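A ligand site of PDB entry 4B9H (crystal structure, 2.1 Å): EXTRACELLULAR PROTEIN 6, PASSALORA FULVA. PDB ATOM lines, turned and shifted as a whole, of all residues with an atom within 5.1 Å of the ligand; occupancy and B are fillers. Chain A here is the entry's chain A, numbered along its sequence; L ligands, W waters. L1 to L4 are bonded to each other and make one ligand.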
ATOM      1  N   VAL A  46      11.799   9.877 -16.558  1.00  0.00           N
ATOM      2  CA  VAL A  46      11.349  11.237 -16.917  1.00  0.00           C
ATOM      3  C   VAL A  46      12.008  12.241 -15.946  1.00  0.00           C
ATOM      4  O   VAL A  46      11.979  12.066 -14.700  1.00  0.00           O
ATOM      5  CB  VAL A  46       9.814  11.321 -16.897  1.00  0.00           C
ATOM      6  CG1 VAL A  46       9.296  12.748 -17.067  1.00  0.00           C
ATOM      7  CG2 VAL A  46       9.224  10.394 -17.980  1.00  0.00           C
ATOM      8  N   VAL A  47      12.649  13.256 -16.528  1.00  0.00           N
ATOM      9  CA  VAL A  47      13.327  14.284 -15.740  1.00  0.00           C
ATOM     10  C   VAL A  47      12.725  15.662 -16.059  1.00  0.00           C
ATOM     11  O   VAL A  47      11.812  15.816 -16.889  1.00  0.00           O
ATOM     12  CB  VAL A  47      14.867  14.271 -15.958  1.00  0.00           C
ATOM     13  CG1 VAL A  47      15.517  12.950 -15.482  1.00  0.00           C
ATOM     14  CG2 VAL A  47      15.255  14.618 -17.414  1.00  0.00           C
ATOM     15  N   LYS A  48      13.240  16.671 -15.386  1.00  0.00           N
ATOM     16  CA  LYS A  48      12.676  18.029 -15.448  1.00  0.00           C
ATOM     17  C   LYS A  48      12.863  18.597 -16.867  1.00  0.00           C
ATOM     18  O   LYS A  48      13.891  18.440 -17.502  1.00  0.00           O
ATOM     19  CB  LYS A  48      13.415  18.908 -14.406  1.00  0.00           C
ATOM     20  CG  LYS A  48      13.273  20.442 -14.582  1.00  0.00           C
ATOM     21  CD  LYS A  48      14.586  21.165 -14.214  1.00  0.00           C
ATOM     22  CE  LYS A  48      14.476  22.683 -14.434  1.00  0.00           C
ATOM     23  NZ  LYS A  48      15.300  23.448 -13.446  1.00  0.00           N
ATOM     24  N   GLY A  49      11.844  19.244 -17.383  1.00  0.00           N
ATOM     25  CA  GLY A  49      11.899  19.792 -18.709  1.00  0.00           C
ATOM     26  C   GLY A  49      11.350  18.822 -19.748  1.00  0.00           C
ATOM     27  O   GLY A  49      11.122  19.232 -20.885  1.00  0.00           O
ATOM     28  N   ASP A  50      11.105  17.554 -19.404  1.00  0.00           N
ATOM     29  CA  ASP A  50      10.802  16.591 -20.463  1.00  0.00           C
ATOM     30  C   ASP A  50       9.393  16.814 -20.956  1.00  0.00           C
ATOM     31  O   ASP A  50       8.479  16.977 -20.163  1.00  0.00           O
ATOM     32  CB  ASP A  50      10.921  15.100 -20.004  1.00  0.00           C
ATOM     33  CG  ASP A  50      12.349  14.599 -19.950  1.00  0.00           C
ATOM     34  OD1 ASP A  50      13.274  15.199 -20.535  1.00  0.00           O
ATOM     35  OD2 ASP A  50      12.541  13.518 -19.346  1.00  0.00           O
ATOM     36  N   THR A  51       9.188  16.744 -22.273  1.00  0.00           N
ATOM     37  CA  THR A  51       7.843  16.421 -22.762  1.00  0.00           C
ATOM     38  C   THR A  51       7.955  15.163 -23.629  1.00  0.00           C
ATOM     39  O   THR A  51       9.072  14.752 -23.982  1.00  0.00           O
ATOM     40  CB  THR A  51       7.234  17.579 -23.565  1.00  0.00           C
ATOM     41  OG1 THR A  51       8.065  17.802 -24.706  1.00  0.00           O
ATOM     42  CG2 THR A  51       7.141  18.901 -22.671  1.00  0.00           C
ATOM     43  N   LEU A  52       6.844  14.574 -24.026  1.00  0.00           N
ATOM     44  CA  LEU A  52       6.919  13.503 -25.054  1.00  0.00           C
ATOM     45  C   LEU A  52       7.592  13.993 -26.340  1.00  0.00           C
ATOM     46  O   LEU A  52       8.350  13.250 -26.966  1.00  0.00           O
ATOM     47  CB  LEU A  52       5.546  12.897 -25.342  1.00  0.00           C
ATOM     48  CG  LEU A  52       5.025  11.954 -24.208  1.00  0.00           C
ATOM     49  CD1 LEU A  52       3.702  11.362 -24.635  1.00  0.00           C
ATOM     50  CD2 LEU A  52       6.065  10.860 -23.894  1.00  0.00           C
ATOM     51  N   THR A  53       7.376  15.275 -26.698  1.00  0.00           N
ATOM     52  CA  THR A  53       8.049  15.829 -27.916  1.00  0.00           C
ATOM     53  C   THR A  53       9.588  15.777 -27.783  1.00  0.00           C
ATOM     54  O   THR A  53      10.258  15.310 -28.671  1.00  0.00           O
ATOM     55  CB  THR A  53       7.593  17.296 -28.235  1.00  0.00           C
ATOM     56  OG1 THR A  53       6.177  17.347 -28.309  1.00  0.00           O
ATOM     57  CG2 THR A  53       8.131  17.729 -29.605  1.00  0.00           C
ATOM     58  N   ILE A  63       6.112  10.476 -30.535  1.00  0.00           N
ATOM     59  CA  ILE A  63       5.182  10.798 -29.467  1.00  0.00           C
ATOM     60  C   ILE A  63       4.134   9.693 -29.299  1.00  0.00           C
ATOM     61  O   ILE A  63       3.968   9.162 -28.208  1.00  0.00           O
ATOM     62  CB  ILE A  63       4.535  12.177 -29.684  1.00  0.00           C
ATOM     63  CG1 ILE A  63       5.624  13.289 -29.683  1.00  0.00           C
ATOM     64  CG2 ILE A  63       3.496  12.484 -28.616  1.00  0.00           C
ATOM     65  CD1 ILE A  63       5.162  14.666 -30.199  1.00  0.00           C
ATOM     66  N   PRO A  75      -1.388  12.258 -23.790  1.00  0.00           N
ATOM     67  CA  PRO A  75      -0.047  12.610 -24.359  1.00  0.00           C
ATOM     68  C   PRO A  75       0.691  13.827 -23.771  1.00  0.00           C
ATOM     69  O   PRO A  75       1.934  13.956 -23.932  1.00  0.00           O
ATOM     70  CB  PRO A  75      -0.348  12.841 -25.844  1.00  0.00           C
ATOM     71  CG  PRO A  75      -1.594  12.030 -26.118  1.00  0.00           C
ATOM     72  CD  PRO A  75      -2.426  12.181 -24.844  1.00  0.00           C
ATOM     73  N   ASN A  76      -0.069  14.748 -23.153  1.00  0.00           N
ATOM     74  CA  ASN A  76       0.523  15.905 -22.521  1.00  0.00           C
ATOM     75  C   ASN A  76       1.064  15.648 -21.111  1.00  0.00           C
ATOM     76  O   ASN A  76       1.798  16.487 -20.604  1.00  0.00           O
ATOM     77  CB  ASN A  76      -0.487  17.092 -22.514  1.00  0.00           C
ATOM     78  CG  ASN A  76      -0.637  17.715 -23.936  1.00  0.00           C
ATOM     79  OD1 ASN A  76       0.197  17.472 -24.802  1.00  0.00           O
ATOM     80  ND2 ASN A  76      -1.680  18.454 -24.160  1.00  0.00           N
ATOM     81  N   LEU A  77       0.713  14.493 -20.511  1.00  0.00           N
ATOM     82  CA  LEU A  77       1.033  14.188 -19.095  1.00  0.00           C
ATOM     83  C   LEU A  77       1.987  13.024 -19.014  1.00  0.00           C
ATOM     84  O   LEU A  77       1.671  11.895 -19.436  1.00  0.00           O
ATOM     85  CB  LEU A  77      -0.257  13.904 -18.299  1.00  0.00           C
ATOM     86  CG  LEU A  77      -0.152  13.425 -16.849  1.00  0.00           C
ATOM     87  CD1 LEU A  77       0.460  14.556 -15.998  1.00  0.00           C
ATOM     88  CD2 LEU A  77      -1.538  12.942 -16.401  1.00  0.00           C
ATOM     89  N   ILE A  78       3.194  13.356 -18.562  1.00  0.00           N
ATOM     90  CA  ILE A  78       4.187  12.361 -18.162  1.00  0.00           C
ATOM     91  C   ILE A  78       4.661  12.851 -16.799  1.00  0.00           C
ATOM     92  O   ILE A  78       4.878  14.049 -16.612  1.00  0.00           O
ATOM     93  CB  ILE A  78       5.375  12.161 -19.180  1.00  0.00           C
ATOM     94  CG1 ILE A  78       6.104  13.461 -19.458  1.00  0.00           C
ATOM     95  CG2 ILE A  78       4.887  11.521 -20.485  1.00  0.00           C
ATOM     96  CD1 ILE A  78       7.245  13.309 -20.453  1.00  0.00           C
ATOM     97  N   GLU A  79       4.833  11.938 -15.863  1.00  0.00           N
ATOM     98  CA  GLU A  79       5.260  12.308 -14.519  1.00  0.00           C
ATOM     99  C   GLU A  79       6.765  12.290 -14.215  1.00  0.00           C
ATOM    100  O   GLU A  79       7.471  11.362 -14.574  1.00  0.00           O
ATOM    101  CB  GLU A  79       4.462  11.498 -13.480  1.00  0.00           C
ATOM    102  CG  GLU A  79       3.170  12.277 -13.139  1.00  0.00           C
ATOM    103  CD  GLU A  79       2.125  11.415 -12.488  1.00  0.00           C
ATOM    104  OE1 GLU A  79       1.882  10.339 -13.020  1.00  0.00           O
ATOM    105  OE2 GLU A  79       1.560  11.785 -11.450  1.00  0.00           O
ATOM    106  N   LEU A  80       7.238  13.348 -13.562  1.00  0.00           N
ATOM    107  CA  LEU A  80       8.584  13.400 -13.080  1.00  0.00           C
ATOM    108  C   LEU A  80       8.919  12.099 -12.347  1.00  0.00           C
ATOM    109  O   LEU A  80       8.158  11.645 -11.447  1.00  0.00           O
ATOM    110  CB  LEU A  80       8.800  14.569 -12.160  1.00  0.00           C
ATOM    111  CG  LEU A  80       9.093  15.892 -12.865  1.00  0.00           C
ATOM    112  CD1 LEU A  80       8.334  17.047 -12.145  1.00  0.00           C
ATOM    113  CD2 LEU A  80      10.624  16.109 -12.953  1.00  0.00           C
ATOM    114  N   VAL A  99      -2.022  13.457 -31.123  1.00  0.00           N
ATOM    115  CA  VAL A  99      -1.928  14.800 -30.605  1.00  0.00           C
ATOM    116  C   VAL A  99      -2.363  15.680 -31.740  1.00  0.00           C
ATOM    117  O   VAL A  99      -2.374  15.246 -32.880  1.00  0.00           O
ATOM    118  CB  VAL A  99      -0.486  15.175 -30.246  1.00  0.00           C
ATOM    119  CG1 VAL A  99       0.094  14.198 -29.236  1.00  0.00           C
ATOM    120  CG2 VAL A  99       0.386  15.217 -31.494  1.00  0.00           C
ATOM    121  N   ASP A 131       2.938  30.711 -24.933  1.00  0.00           N
ATOM    122  CA  ASP A 131       1.949  30.486 -23.857  1.00  0.00           C
ATOM    123  C   ASP A 131       0.752  31.425 -23.961  1.00  0.00           C
ATOM    124  O   ASP A 131      -0.353  31.061 -23.634  1.00  0.00           O
ATOM    125  CB  ASP A 131       2.614  30.704 -22.475  1.00  0.00           C
ATOM    126  CG  ASP A 131       3.573  29.575 -22.099  1.00  0.00           C
ATOM    127  OD1 ASP A 131       3.503  28.502 -22.725  1.00  0.00           O
ATOM    128  OD2 ASP A 131       4.315  29.762 -21.117  1.00  0.00           O
ATOM    129  N   ILE A 176      -7.183  21.638  -8.263  1.00  0.00           N
ATOM    130  CA  ILE A 176      -6.462  20.714  -9.158  1.00  0.00           C
ATOM    131  C   ILE A 176      -6.966  19.292  -8.897  1.00  0.00           C
ATOM    132  O   ILE A 176      -7.165  18.919  -7.739  1.00  0.00           O
ATOM    133  CB  ILE A 176      -4.928  20.827  -8.940  1.00  0.00           C
ATOM    134  CG1 ILE A 176      -4.403  22.162  -9.523  1.00  0.00           C
ATOM    135  CG2 ILE A 176      -4.179  19.675  -9.551  1.00  0.00           C
ATOM    136  CD1 ILE A 176      -4.732  22.402 -10.986  1.00  0.00           C
ATOM    137  N   VAL A 177      -7.276  18.540  -9.951  1.00  0.00           N
ATOM    138  CA  VAL A 177      -7.585  17.114  -9.795  1.00  0.00           C
ATOM    139  C   VAL A 177      -6.454  16.325 -10.485  1.00  0.00           C
ATOM    140  O   VAL A 177      -5.645  16.902 -11.223  1.00  0.00           O
ATOM    141  CB  VAL A 177      -8.984  16.691 -10.351  1.00  0.00           C
ATOM    142  CG1 VAL A 177     -10.158  17.316  -9.545  1.00  0.00           C
ATOM    143  CG2 VAL A 177      -9.098  16.994 -11.837  1.00  0.00           C
ATOM    144  N   ALA A 178      -6.397  15.009 -10.227  1.00  0.00           N
ATOM    145  CA  ALA A 178      -5.280  14.159 -10.683  1.00  0.00           C
ATOM    146  C   ALA A 178      -5.140  14.263 -12.212  1.00  0.00           C
ATOM    147  O   ALA A 178      -6.140  14.160 -12.936  1.00  0.00           O
ATOM    148  CB  ALA A 178      -5.533  12.698 -10.253  1.00  0.00           C
ATOM    149  N   GLY A 179      -3.921  14.474 -12.711  1.00  0.00           N
ATOM    150  CA  GLY A 179      -3.722  14.662 -14.156  1.00  0.00           C
ATOM    151  C   GLY A 179      -4.040  16.083 -14.711  1.00  0.00           C
ATOM    152  O   GLY A 179      -3.981  16.305 -15.925  1.00  0.00           O
ATOM    153  N   ASP A 180      -4.410  17.037 -13.877  1.00  0.00           N
ATOM    154  CA  ASP A 180      -4.600  18.413 -14.400  1.00  0.00           C
ATOM    155  C   ASP A 180      -3.269  19.063 -14.835  1.00  0.00           C
ATOM    156  O   ASP A 180      -2.302  18.965 -14.138  1.00  0.00           O
ATOM    157  CB  ASP A 180      -5.292  19.320 -13.389  1.00  0.00           C
ATOM    158  CG  ASP A 180      -6.777  19.245 -13.478  1.00  0.00           C
ATOM    159  OD1 ASP A 180      -7.258  18.641 -14.433  1.00  0.00           O
ATOM    160  OD2 ASP A 180      -7.469  19.808 -12.620  1.00  0.00           O
ATOM    161  N   LEU A 181      -3.311  19.716 -16.004  1.00  0.00           N
ATOM    162  CA  LEU A 181      -2.204  20.478 -16.588  1.00  0.00           C
ATOM    163  C   LEU A 181      -2.746  21.840 -17.110  1.00  0.00           C
ATOM    164  O   LEU A 181      -3.859  21.903 -17.656  1.00  0.00           O
ATOM    165  CB  LEU A 181      -1.576  19.697 -17.775  1.00  0.00           C
ATOM    166  CG  LEU A 181      -0.857  18.370 -17.507  1.00  0.00           C
ATOM    167  CD1 LEU A 181      -0.312  17.824 -18.831  1.00  0.00           C
ATOM    168  CD2 LEU A 181       0.259  18.493 -16.468  1.00  0.00           C
ATOM    169  N   PHE A 182      -1.969  22.898 -16.880  1.00  0.00           N
ATOM    170  CA  PHE A 182      -2.193  24.246 -17.461  1.00  0.00           C
ATOM    171  C   PHE A 182      -2.525  24.166 -18.962  1.00  0.00           C
ATOM    172  O   PHE A 182      -3.532  24.789 -19.398  1.00  0.00           O
ATOM    173  CB  PHE A 182      -0.963  25.204 -17.230  1.00  0.00           C
ATOM    174  CG  PHE A 182      -0.792  25.767 -15.825  1.00  0.00           C
ATOM    175  CD1 PHE A 182      -1.503  25.282 -14.736  1.00  0.00           C
ATOM    176  CD2 PHE A 182       0.070  26.820 -15.596  1.00  0.00           C
ATOM    177  CE1 PHE A 182      -1.340  25.789 -13.461  1.00  0.00           C
ATOM    178  CE2 PHE A 182       0.272  27.316 -14.299  1.00  0.00           C
ATOM    179  CZ  PHE A 182      -0.452  26.813 -13.240  1.00  0.00           C
ATOM    180  N   VAL A 183      -1.718  23.410 -19.737  1.00  0.00           N
ATOM    181  CA  VAL A 183      -1.986  23.229 -21.203  1.00  0.00           C
ATOM    182  C   VAL A 183      -3.419  22.742 -21.475  1.00  0.00           C
ATOM    183  O   VAL A 183      -4.156  23.318 -22.325  1.00  0.00           O
ATOM    184  CB  VAL A 183      -0.962  22.293 -21.910  1.00  0.00           C
ATOM    185  CG1 VAL A 183      -0.874  20.895 -21.236  1.00  0.00           C
ATOM    186  CG2 VAL A 183      -1.250  22.180 -23.449  1.00  0.00           C
ATOM    187  N   ILE A 193      -2.421  29.142 -21.507  1.00  0.00           N
ATOM    188  CA  ILE A 193      -1.384  28.851 -20.562  1.00  0.00           C
ATOM    189  C   ILE A 193      -0.867  30.135 -19.891  1.00  0.00           C
ATOM    190  O   ILE A 193      -0.688  30.172 -18.643  1.00  0.00           O
ATOM    191  CB  ILE A 193      -0.188  28.097 -21.219  1.00  0.00           C
ATOM    192  CG1 ILE A 193      -0.562  26.663 -21.669  1.00  0.00           C
ATOM    193  CG2 ILE A 193       0.995  28.122 -20.251  1.00  0.00           C
ATOM    194  CD1 ILE A 193       0.406  25.958 -22.661  1.00  0.00           C
ATOM    195  N   LYS A 197      -0.770  31.158 -15.966  1.00  0.00           N
ATOM    196  CA  LYS A 197       0.497  31.471 -15.340  1.00  0.00           C
ATOM    197  C   LYS A 197       0.501  32.857 -14.721  1.00  0.00           C
ATOM    198  O   LYS A 197       1.026  33.005 -13.601  1.00  0.00           O
ATOM    199  CB  LYS A 197       1.738  31.297 -16.277  1.00  0.00           C
ATOM    200  CG  LYS A 197       2.020  29.912 -16.813  1.00  0.00           C
ATOM    201  CD  LYS A 197       3.229  29.963 -17.775  1.00  0.00           C
ATOM    202  CE  LYS A 197       3.932  28.595 -17.828  1.00  0.00           C
ATOM    203  NZ  LYS A 197       5.110  28.523 -18.744  1.00  0.00           N
ATOM    204  N   ASN A 204       4.798  26.722 -10.160  1.00  0.00           N
ATOM    205  CA  ASN A 204       5.500  25.966 -11.187  1.00  0.00           C
ATOM    206  C   ASN A 204       4.450  24.975 -11.774  1.00  0.00           C
ATOM    207  O   ASN A 204       3.772  24.227 -11.030  1.00  0.00           O
ATOM    208  CB  ASN A 204       6.735  25.307 -10.562  1.00  0.00           C
ATOM    209  CG  ASN A 204       7.571  24.498 -11.558  1.00  0.00           C
ATOM    210  OD1 ASN A 204       7.051  23.904 -12.472  1.00  0.00           O
ATOM    211  ND2 ASN A 204       8.848  24.429 -11.316  1.00  0.00           N
ATOM    212  N   PRO A 205       4.215  25.030 -13.091  1.00  0.00           N
ATOM    213  CA  PRO A 205       3.175  24.135 -13.596  1.00  0.00           C
ATOM    214  C   PRO A 205       3.477  22.636 -13.418  1.00  0.00           C
ATOM    215  O   PRO A 205       2.571  21.807 -13.610  1.00  0.00           O
ATOM    216  CB  PRO A 205       3.132  24.434 -15.085  1.00  0.00           C
ATOM    217  CG  PRO A 205       3.797  25.761 -15.263  1.00  0.00           C
ATOM    218  CD  PRO A 205       4.766  25.923 -14.142  1.00  0.00           C
ATOM    219  N   SER A 206       4.755  22.318 -13.163  1.00  0.00           N
ATOM    220  CA  SER A 206       5.255  20.937 -13.129  1.00  0.00           C
ATOM    221  C   SER A 206       5.191  20.383 -11.709  1.00  0.00           C
ATOM    222  O   SER A 206       5.519  19.235 -11.480  1.00  0.00           O
ATOM    223  CB  SER A 206       6.685  20.873 -13.684  1.00  0.00           C
ATOM    224  OG  SER A 206       6.580  20.794 -15.089  1.00  0.00           O
ATOM    225  N   LYS A 207       4.719  21.193 -10.782  1.00  0.00           N
ATOM    226  CA  LYS A 207       4.673  20.796  -9.375  1.00  0.00           C
ATOM    227  C   LYS A 207       3.256  20.957  -8.781  1.00  0.00           C
ATOM    228  O   LYS A 207       3.110  21.334  -7.641  1.00  0.00           O
ATOM    229  CB  LYS A 207       5.723  21.625  -8.592  1.00  0.00           C
ATOM    230  CG  LYS A 207       7.153  21.361  -9.062  1.00  0.00           C
ATOM    231  CD  LYS A 207       8.223  21.990  -8.179  1.00  0.00           C
ATOM    232  CE  LYS A 207       9.610  21.643  -8.741  1.00  0.00           C
ATOM    233  NZ  LYS A 207      10.780  22.220  -7.995  1.00  0.00           N
ATOM    234  N   LEU A 208       2.213  20.724  -9.572  1.00  0.00           N
ATOM    235  CA  LEU A 208       0.854  20.813  -9.073  1.00  0.00           C
ATOM    236  C   LEU A 208       0.473  19.540  -8.286  1.00  0.00           C
ATOM    237  O   LEU A 208       0.847  18.415  -8.667  1.00  0.00           O
ATOM    238  CB  LEU A 208      -0.165  20.978 -10.205  1.00  0.00           C
ATOM    239  CG  LEU A 208       0.041  22.128 -11.172  1.00  0.00           C
ATOM    240  CD1 LEU A 208      -0.849  22.022 -12.390  1.00  0.00           C
ATOM    241  CD2 LEU A 208      -0.080  23.465 -10.427  1.00  0.00           C
ATOM    242  N   LYS A 209      -0.321  19.715  -7.235  1.00  0.00           N
ATOM    243  CA  LYS A 209      -0.710  18.596  -6.335  1.00  0.00           C
ATOM    244  C   LYS A 209      -2.251  18.486  -6.326  1.00  0.00           C
ATOM    245  O   LYS A 209      -2.938  19.511  -6.370  1.00  0.00           O
ATOM    246  CB  LYS A 209      -0.150  18.864  -4.926  1.00  0.00           C
ATOM    247  CG  LYS A 209       1.361  19.091  -4.862  1.00  0.00           C
ATOM    248  CD  LYS A 209       2.120  17.944  -4.207  1.00  0.00           C
ATOM    249  CE  LYS A 209       3.604  18.262  -4.058  1.00  0.00           C
ATOM    250  NZ  LYS A 209       4.310  17.227  -3.237  1.00  0.00           N
ATOM    251  N   VAL A 210      -2.784  17.262  -6.295  1.00  0.00           N
ATOM    252  CA  VAL A 210      -4.236  17.075  -6.260  1.00  0.00           C
ATOM    253  C   VAL A 210      -4.716  17.894  -5.082  1.00  0.00           C
ATOM    254  O   VAL A 210      -4.022  17.943  -4.052  1.00  0.00           O
ATOM    255  CB  VAL A 210      -4.665  15.585  -6.112  1.00  0.00           C
ATOM    256  CG1 VAL A 210      -6.162  15.477  -5.805  1.00  0.00           C
ATOM    257  CG2 VAL A 210      -4.324  14.787  -7.377  1.00  0.00           C
HETATM  258  C1  LIG L   1       3.052  20.397 -25.271  1.00  0.00           C
HETATM  259  C2  LIG L   1       3.534  19.099 -24.571  1.00  0.00           C
HETATM  260  C3  LIG L   1       3.121  19.078 -23.090  1.00  0.00           C
HETATM  261  C4  LIG L   1       3.606  20.345 -22.409  1.00  0.00           C
HETATM  262  C5  LIG L   1       3.190  21.586 -23.187  1.00  0.00           C
HETATM  263  C6  LIG L   1       3.840  22.821 -22.550  1.00  0.00           C
HETATM  264  C7  LIG L   1       3.788  17.050 -25.949  1.00  0.00           C
HETATM  265  C8  LIG L   1       3.086  15.879 -26.644  1.00  0.00           C
HETATM  266  O1  LIG L   1       3.551  21.548 -24.568  1.00  0.00           O
HETATM  267  O2  LIG L   1       3.610  17.952 -22.345  1.00  0.00           O
HETATM  268  O3  LIG L   1       2.973  20.406 -21.154  1.00  0.00           O
HETATM  269  O4  LIG L   1       2.945  23.874 -22.785  1.00  0.00           O
HETATM  270  O5  LIG L   1       5.039  17.201 -26.014  1.00  0.00           O
HETATM  271  N1  LIG L   1       3.004  17.934 -25.273  1.00  0.00           N
HETATM  272  O6  LIG L   1       1.624  20.445 -25.218  1.00  0.00           O
HETATM  273  C1  LG2 L   2       3.765  20.129 -20.009  1.00  0.00           C
HETATM  274  C2  LG2 L   2       3.070  20.822 -18.822  1.00  0.00           C
HETATM  275  C3  LG2 L   2       3.693  20.431 -17.453  1.00  0.00           C
HETATM  276  C4  LG2 L   2       3.942  18.941 -17.386  1.00  0.00           C
HETATM  277  C5  LG2 L   2       4.632  18.402 -18.655  1.00  0.00           C
HETATM  278  C6  LG2 L   2       4.774  16.877 -18.617  1.00  0.00           C
HETATM  279  C7  LG2 L   2       2.008  23.054 -18.907  1.00  0.00           C
HETATM  280  C8  LG2 L   2       2.287  24.542 -19.044  1.00  0.00           C
HETATM  281  N1  LG2 L   2       3.095  22.277 -18.962  1.00  0.00           N
HETATM  282  O1  LG2 L   2       2.950  20.928 -16.358  1.00  0.00           O
HETATM  283  O2  LG2 L   2       4.786  18.654 -16.282  1.00  0.00           O
HETATM  284  O3  LG2 L   2       3.830  18.720 -19.786  1.00  0.00           O
HETATM  285  O4  LG2 L   2       3.467  16.355 -18.529  1.00  0.00           O
HETATM  286  O5  LG2 L   2       0.886  22.603 -18.724  1.00  0.00           O
HETATM  287  C1  LG3 L   3       4.104  17.759 -15.357  1.00  0.00           C
HETATM  288  C2  LG3 L   3       5.114  17.019 -14.468  1.00  0.00           C
HETATM  289  C3  LG3 L   3       4.395  16.102 -13.481  1.00  0.00           C
HETATM  290  C4  LG3 L   3       3.286  16.886 -12.801  1.00  0.00           C
HETATM  291  C5  LG3 L   3       2.388  17.674 -13.753  1.00  0.00           C
HETATM  292  C6  LG3 L   3       1.459  18.633 -12.970  1.00  0.00           C
HETATM  293  C7  LG3 L   3       7.250  16.814 -15.620  1.00  0.00           C
HETATM  294  C8  LG3 L   3       8.172  16.005 -16.475  1.00  0.00           C
HETATM  295  N1  LG3 L   3       6.059  16.260 -15.280  1.00  0.00           N
HETATM  296  O1  LG3 L   3       5.323  15.511 -12.547  1.00  0.00           O
HETATM  297  O2  LG3 L   3       2.366  16.011 -12.289  1.00  0.00           O
HETATM  298  O3  LG3 L   3       3.184  18.500 -14.602  1.00  0.00           O
HETATM  299  O4  LG3 L   3       2.238  19.544 -12.170  1.00  0.00           O
HETATM  300  O5  LG3 L   3       7.595  17.934 -15.219  1.00  0.00           O
HETATM  301  C1  LG4 L   4       2.525  15.684 -10.925  1.00  0.00           C
HETATM  302  C2  LG4 L   4       1.172  15.303 -10.336  1.00  0.00           C
HETATM  303  C3  LG4 L   4       1.412  14.708  -8.923  1.00  0.00           C
HETATM  304  C4  LG4 L   4       2.473  13.606  -8.923  1.00  0.00           C
HETATM  305  C5  LG4 L   4       3.756  14.115  -9.612  1.00  0.00           C
HETATM  306  C6  LG4 L   4       4.877  13.059  -9.737  1.00  0.00           C
HETATM  307  C7  LG4 L   4      -1.076  16.284 -11.061  1.00  0.00           C
HETATM  308  C8  LG4 L   4      -2.066  17.422 -10.952  1.00  0.00           C
HETATM  309  N1  LG4 L   4       0.106  16.348 -10.348  1.00  0.00           N
HETATM  310  O1  LG4 L   4       0.208  14.264  -8.317  1.00  0.00           O
HETATM  311  O2  LG4 L   4       2.745  13.239  -7.591  1.00  0.00           O
HETATM  312  O3  LG4 L   4       3.459  14.602 -10.912  1.00  0.00           O
HETATM  313  O4  LG4 L   4       5.943  13.623 -10.489  1.00  0.00           O
HETATM  314  O5  LG4 L   4      -1.400  15.342 -11.801  1.00  0.00           O
HETATM  315  O   HOH W   1       4.400  26.196 -21.881  1.00  0.00           O
HETATM  316  O   HOH W   2       4.210  15.327 -22.959  1.00  0.00           O
HETATM  317  O   HOH W   3       5.700  23.474 -18.962  1.00  0.00           O
HETATM  318  O   HOH W   4       5.232  26.148 -19.542  1.00  0.00           O
HETATM  319  O   HOH W   5       0.690  22.335 -15.723  1.00  0.00           O
HETATM  320  O   HOH W   6      -0.399  15.071  -5.811  1.00  0.00           O
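The backbone NH (N) of Thr 53 is in hydrogen-bond range of an oxygen (O5) of LIG L1 (3.1 Å).
The side-chain hydroxyl of Thr 53 is in hydrogen-bond range of an oxygen (O5) of LIG L1 (2.6 Å).
An oxygen (O4) of LG2 L2 lies within hydrogen-bond range of the backbone carbonyl oxygen of Asn 76 (2.7 Å).
N1 of LIG L1 sits at hydrogen-bond distance from OD1 of Asn 76, at 2.9 Å.
An oxygen (O4) of LG3 L3 lies within hydrogen-bond range of the backbone carbonyl oxygen of Pro 205 (2.7 Å).
N of Leu 208 sits at hydrogen-bond distance from O4 of LG3 L3 (2.9 Å).
O of Leu 208 is in hydrogen-bond range of N1 of LG4 L4 (2.8 Å).
The backbone NH of Gly 179 lies within hydrogen-bond range of an oxygen (O5) of LG4 L4, at 2.8 Å.
The backbone NH (N) of Ile 78 lies within hydrogen-bond range of an oxygen (O4) of LG2 L2, at 3.0 Å.
The backbone carbonyl oxygen (O) of Ile 78 lies within hydrogen-bond range of a nitrogen (N1) of LG3 L3, 2.8 Å away.
O5 of LG2 L2 lies within hydrogen-bond range of N of Val 183.
An oxygen (O4) of LG3 L3 lies close to the backbone carbonyl oxygen (O) of Ser 206.
An oxygen (O2) of LG2 L2 sits at hydrogen-bond distance from the side-chain hydroxyl (OG) of Ser 206 (3.0 Å).
N of Leu 80 lies within hydrogen-bond range of O1 of LG3 L3 (3.1 Å).
O of Leu 80 sits at hydrogen-bond distance from O4 of LG4 L4 (3.1 Å).
The backbone NH (N) of Lys 207 lies within hydrogen-bond range of an oxygen (O4) of LG3 L3 (3.3 Å).
O5 of LIG L1 lies close to OG1 of Thr 51, at 3.4 Å.
The backbone NH (N) of Phe 182 is in hydrogen-bond range of an oxygen (O5) of LG2 L2, at 3.4 Å.
The backbone NH (N) of Thr 53 sits close to the side-chain hydroxyl (OG1) of Thr 51 (3.3 Å).
The side-chain amide oxygen (OD1) of Asn 204 lies within hydrogen-bond range of the backbone NH (N) of Ser 206, at 2.9 Å.
The backbone NH (N) of Val 177 is in hydrogen-bond range of the side-chain carboxylate (OD2) of Asp 180, 3.0 Å away.
The side-chain carboxylate of Asp 50 sits at hydrogen-bond distance from the backbone NH of Val 47 (2.8 Å).
An oxygen (O3) of LG4 L4 sits close to the side-chain carboxylate (OE2) of Glu 79.
Residues that only touch the ligand: Ile 193 (3.3 Å), Leu 77 (3.3 Å), Ile 176 (3.4 Å), Leu 181 (3.5 Å), Val 46 (3.5 Å), Pro 75 (3.5 Å), Asp 180 (3.5 Å), Val 177 (3.6 Å), Val 47 (3.7 Å), Leu 52 (3.8 Å), Asp 50 (3.8 Å), Ala 178 (3.9 Å) and Ile 63 (3.9 Å).
Hydrophobic or aromatic side chains that line the ligand: Val 46, Ile 63, Ile 78, Leu 80, Ile 176, Leu 181, Phe 182, Val 183, Ile 193, Pro 205 and Leu 208.
Of the 34 residues printed, 26 come within 4 Å of the ligand.
Water W6 lies within hydrogen-bond range of an oxygen (O1) of LG4 L4 and the backbone NH (N) of Val 210.
Water W5 lies within hydrogen-bond range of O1 of LG2 L2 (2.7 Å), O of Pro 205 (2.9 Å) and N of Phe 182 (3.0 Å).
Water W2 lies within hydrogen-bond range of an oxygen (O2) of LIG L1, the backbone carbonyl oxygen of Pro 75 and the backbone NH of Leu 52.
Water W1 bridges the side-chain carboxylate of Asp 131 and an oxygen (O4) of LIG L1.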
